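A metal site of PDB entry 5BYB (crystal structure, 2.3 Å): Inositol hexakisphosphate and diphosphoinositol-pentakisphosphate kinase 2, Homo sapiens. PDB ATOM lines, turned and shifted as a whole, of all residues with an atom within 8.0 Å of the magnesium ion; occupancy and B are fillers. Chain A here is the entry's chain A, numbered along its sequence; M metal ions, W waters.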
ATOM      1  N   GLN A   7      12.446  27.648 -12.618  1.00  0.00           N
ATOM      2  CA  GLN A   7      13.743  26.911 -12.604  1.00  0.00           C
ATOM      3  C   GLN A   7      13.849  26.013 -13.819  1.00  0.00           C
ATOM      4  O   GLN A   7      12.879  25.406 -14.221  1.00  0.00           O
ATOM      5  CB  GLN A   7      13.868  26.063 -11.334  1.00  0.00           C
ATOM      6  CG  GLN A   7      14.161  26.837 -10.063  1.00  0.00           C
ATOM      7  CD  GLN A   7      15.631  27.170  -9.908  1.00  0.00           C
ATOM      8  OE1 GLN A   7      16.507  26.297  -9.964  1.00  0.00           O
ATOM      9  NE2 GLN A   7      15.923  28.440  -9.746  1.00  0.00           N
ATOM     10  N   ILE A   8      15.024  25.964 -14.424  1.00  0.00           N
ATOM     11  CA  ILE A   8      15.246  25.022 -15.508  1.00  0.00           C
ATOM     12  C   ILE A   8      15.654  23.708 -14.838  1.00  0.00           C
ATOM     13  O   ILE A   8      16.470  23.704 -13.937  1.00  0.00           O
ATOM     14  CB  ILE A   8      16.315  25.546 -16.498  1.00  0.00           C
ATOM     15  CG1 ILE A   8      15.800  26.831 -17.171  1.00  0.00           C
ATOM     16  CG2 ILE A   8      16.645  24.517 -17.568  1.00  0.00           C
ATOM     17  CD1 ILE A   8      16.895  27.756 -17.652  1.00  0.00           C
ATOM     18  N   LEU A  28      27.598  17.765 -10.622  1.00  0.00           N
ATOM     19  CA  LEU A  28      26.226  18.151 -10.325  1.00  0.00           C
ATOM     20  C   LEU A  28      26.151  19.215  -9.238  1.00  0.00           C
ATOM     21  O   LEU A  28      25.314  20.120  -9.288  1.00  0.00           O
ATOM     22  CB  LEU A  28      25.399  16.928  -9.934  1.00  0.00           C
ATOM     23  CG  LEU A  28      25.288  15.849 -11.012  1.00  0.00           C
ATOM     24  CD1 LEU A  28      24.260  14.826 -10.566  1.00  0.00           C
ATOM     25  CD2 LEU A  28      24.958  16.435 -12.401  1.00  0.00           C
ATOM     26  N   GLU A  29      27.027  19.112  -8.255  1.00  0.00           N
ATOM     27  CA  GLU A  29      27.033  20.099  -7.178  1.00  0.00           C
ATOM     28  C   GLU A  29      27.398  21.496  -7.701  1.00  0.00           C
ATOM     29  O   GLU A  29      26.906  22.490  -7.195  1.00  0.00           O
ATOM     30  CB  GLU A  29      27.997  19.621  -6.108  1.00  0.00           C
ATOM     31  CG  GLU A  29      28.689  20.643  -5.226  1.00  0.00           C
ATOM     32  CD  GLU A  29      29.855  19.992  -4.533  1.00  0.00           C
ATOM     33  OE1 GLU A  29      29.771  19.732  -3.323  1.00  0.00           O
ATOM     34  OE2 GLU A  29      30.855  19.658  -5.216  1.00  0.00           O
ATOM     35  N   ARG A  30      28.266  21.554  -8.724  1.00  0.00           N
ATOM     36  CA  ARG A  30      28.650  22.838  -9.295  1.00  0.00           C
ATOM     37  C   ARG A  30      27.587  23.360 -10.280  1.00  0.00           C
ATOM     38  O   ARG A  30      27.281  24.561 -10.310  1.00  0.00           O
ATOM     39  CB  ARG A  30      30.025  22.792  -9.936  1.00  0.00           C
ATOM     40  CG  ARG A  30      31.180  22.478  -8.997  1.00  0.00           C
ATOM     41  CD  ARG A  30      32.389  22.001  -9.826  1.00  0.00           C
ATOM     42  NE  ARG A  30      33.672  21.960  -9.119  1.00  0.00           N
ATOM     43  CZ  ARG A  30      33.999  21.059  -8.180  1.00  0.00           C
ATOM     44  NH1 ARG A  30      33.126  20.130  -7.796  1.00  0.00           N
ATOM     45  NH2 ARG A  30      35.205  21.098  -7.630  1.00  0.00           N
ATOM     46  N   ILE A  31      27.004  22.455 -11.069  1.00  0.00           N
ATOM     47  CA  ILE A  31      25.894  22.823 -11.972  1.00  0.00           C
ATOM     48  C   ILE A  31      24.743  23.431 -11.151  1.00  0.00           C
ATOM     49  O   ILE A  31      24.129  24.425 -11.576  1.00  0.00           O
ATOM     50  CB  ILE A  31      25.383  21.631 -12.835  1.00  0.00           C
ATOM     51  CG1 ILE A  31      26.402  21.244 -13.931  1.00  0.00           C
ATOM     52  CG2 ILE A  31      24.031  21.949 -13.484  1.00  0.00           C
ATOM     53  CD1 ILE A  31      26.021  19.968 -14.673  1.00  0.00           C
ATOM     54  N   SER A  32      24.472  22.837  -9.990  1.00  0.00           N
ATOM     55  CA  SER A  32      23.460  23.336  -9.054  1.00  0.00           C
ATOM     56  C   SER A  32      23.675  24.781  -8.586  1.00  0.00           C
ATOM     57  O   SER A  32      22.700  25.456  -8.219  1.00  0.00           O
ATOM     58  CB  SER A  32      23.324  22.409  -7.846  1.00  0.00           C
ATOM     59  OG  SER A  32      22.617  21.239  -8.183  1.00  0.00           O
ATOM     60  N   LEU A  33      24.923  25.268  -8.600  1.00  0.00           N
ATOM     61  CA  LEU A  33      25.194  26.669  -8.249  1.00  0.00           C
ATOM     62  C   LEU A  33      24.636  27.668  -9.267  1.00  0.00           C
ATOM     63  O   LEU A  33      24.601  28.880  -9.003  1.00  0.00           O
ATOM     64  CB  LEU A  33      26.696  26.945  -8.066  1.00  0.00           C
ATOM     65  CG  LEU A  33      27.476  26.128  -7.018  1.00  0.00           C
ATOM     66  CD1 LEU A  33      28.983  26.308  -7.190  1.00  0.00           C
ATOM     67  CD2 LEU A  33      27.061  26.407  -5.566  1.00  0.00           C
ATOM     68  N   PHE A  34      24.222  27.172 -10.431  1.00  0.00           N
ATOM     69  CA  PHE A  34      23.469  28.016 -11.360  1.00  0.00           C
ATOM     70  C   PHE A  34      22.110  28.366 -10.708  1.00  0.00           C
ATOM     71  O   PHE A  34      21.320  27.476 -10.296  1.00  0.00           O
ATOM     72  CB  PHE A  34      23.301  27.357 -12.721  1.00  0.00           C
ATOM     73  CG  PHE A  34      24.497  27.514 -13.634  1.00  0.00           C
ATOM     74  CD1 PHE A  34      25.703  26.839 -13.379  1.00  0.00           C
ATOM     75  CD2 PHE A  34      24.417  28.338 -14.776  1.00  0.00           C
ATOM     76  CE1 PHE A  34      26.796  26.992 -14.239  1.00  0.00           C
ATOM     77  CE2 PHE A  34      25.513  28.483 -15.630  1.00  0.00           C
ATOM     78  CZ  PHE A  34      26.695  27.816 -15.349  1.00  0.00           C
ATOM     79  N   LYS A  35      21.863  29.674 -10.613  1.00  0.00           N
ATOM     80  CA  LYS A  35      20.703  30.211  -9.929  1.00  0.00           C
ATOM     81  C   LYS A  35      19.376  29.742 -10.541  1.00  0.00           C
ATOM     82  O   LYS A  35      18.396  29.508  -9.812  1.00  0.00           O
ATOM     83  CB  LYS A  35      20.798  31.745  -9.902  1.00  0.00           C
ATOM     84  CG  LYS A  35      19.553  32.465  -9.425  1.00  0.00           C
ATOM     85  CD  LYS A  35      19.766  33.968  -9.380  1.00  0.00           C
ATOM     86  CE  LYS A  35      18.475  34.664  -8.969  1.00  0.00           C
ATOM     87  NZ  LYS A  35      18.359  35.997  -9.629  1.00  0.00           N
ATOM     88  N   TYR A  36      19.325  29.553 -11.853  1.00  0.00           N
ATOM     89  CA  TYR A  36      18.069  29.154 -12.458  1.00  0.00           C
ATOM     90  C   TYR A  36      17.995  27.686 -12.779  1.00  0.00           C
ATOM     91  O   TYR A  36      17.032  27.242 -13.431  1.00  0.00           O
ATOM     92  CB  TYR A  36      17.783  29.977 -13.709  1.00  0.00           C
ATOM     93  CG  TYR A  36      17.603  31.441 -13.399  1.00  0.00           C
ATOM     94  CD1 TYR A  36      16.396  31.917 -12.875  1.00  0.00           C
ATOM     95  CD2 TYR A  36      18.647  32.351 -13.609  1.00  0.00           C
ATOM     96  CE1 TYR A  36      16.228  33.259 -12.584  1.00  0.00           C
ATOM     97  CE2 TYR A  36      18.485  33.704 -13.324  1.00  0.00           C
ATOM     98  CZ  TYR A  36      17.271  34.142 -12.814  1.00  0.00           C
ATOM     99  OH  TYR A  36      17.103  35.484 -12.524  1.00  0.00           O
ATOM    100  N   ILE A  37      18.982  26.925 -12.315  1.00  0.00           N
ATOM    101  CA  ILE A  37      19.022  25.497 -12.603  1.00  0.00           C
ATOM    102  C   ILE A  37      18.747  24.661 -11.369  1.00  0.00           C
ATOM    103  O   ILE A  37      19.332  24.920 -10.279  1.00  0.00           O
ATOM    104  CB  ILE A  37      20.353  25.078 -13.265  1.00  0.00           C
ATOM    105  CG1 ILE A  37      20.411  25.593 -14.703  1.00  0.00           C
ATOM    106  CG2 ILE A  37      20.492  23.572 -13.311  1.00  0.00           C
ATOM    107  CD1 ILE A  37      21.761  25.441 -15.356  1.00  0.00           C
ATOM    108  N   THR A  38      17.846  23.682 -11.515  1.00  0.00           N
ATOM    109  CA  THR A  38      17.674  22.605 -10.531  1.00  0.00           C
ATOM    110  C   THR A  38      18.019  21.278 -11.185  1.00  0.00           C
ATOM    111  O   THR A  38      17.585  20.982 -12.284  1.00  0.00           O
ATOM    112  CB  THR A  38      16.214  22.497 -10.016  1.00  0.00           C
ATOM    113  OG1 THR A  38      15.776  23.777  -9.528  1.00  0.00           O
ATOM    114  CG2 THR A  38      16.085  21.460  -8.882  1.00  0.00           C
ATOM    115  N   VAL A  39      18.786  20.467 -10.462  1.00  0.00           N
ATOM    116  CA  VAL A  39      19.275  19.196 -10.946  1.00  0.00           C
ATOM    117  C   VAL A  39      18.428  18.100 -10.316  1.00  0.00           C
ATOM    118  O   VAL A  39      18.245  18.081  -9.103  1.00  0.00           O
ATOM    119  CB  VAL A  39      20.750  18.989 -10.505  1.00  0.00           C
ATOM    120  CG1 VAL A  39      21.227  17.562 -10.780  1.00  0.00           C
ATOM    121  CG2 VAL A  39      21.656  20.005 -11.194  1.00  0.00           C
HETATM  122 MG    MG M   1      20.666  25.948  -8.854  1.00  0.00          MG
HETATM  123  O   HOH W   1      19.702  24.342  -7.331  1.00  0.00           O
HETATM  124  O   HOH W   2      21.100  27.905  -7.104  1.00  0.00           O
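The magnesium ion is bound by the backbone carbonyl oxygen of Ser 32, the backbone carbonyl oxygen of Phe 34, the backbone carbonyl oxygen of Ile 37 and water W1.
Slightly farther from the magnesium ion lies water W2 (2.7 Å).
Of the 14 residues printed, 3 come within 4 Å of the magnesium ion.
The nearest printed residue that does not touch the magnesium ion is Lys 35 (4.3 Å).
The backbone carbonyl oxygen of Leu 28 lies within hydrogen-bond range of the side-chain hydroxyl of Ser 32, 3.1 Å away.
The side-chain amide oxygen (OE1) of Gln 7 lies close to the backbone NH (N) of Ile 37 (3.5 Å).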
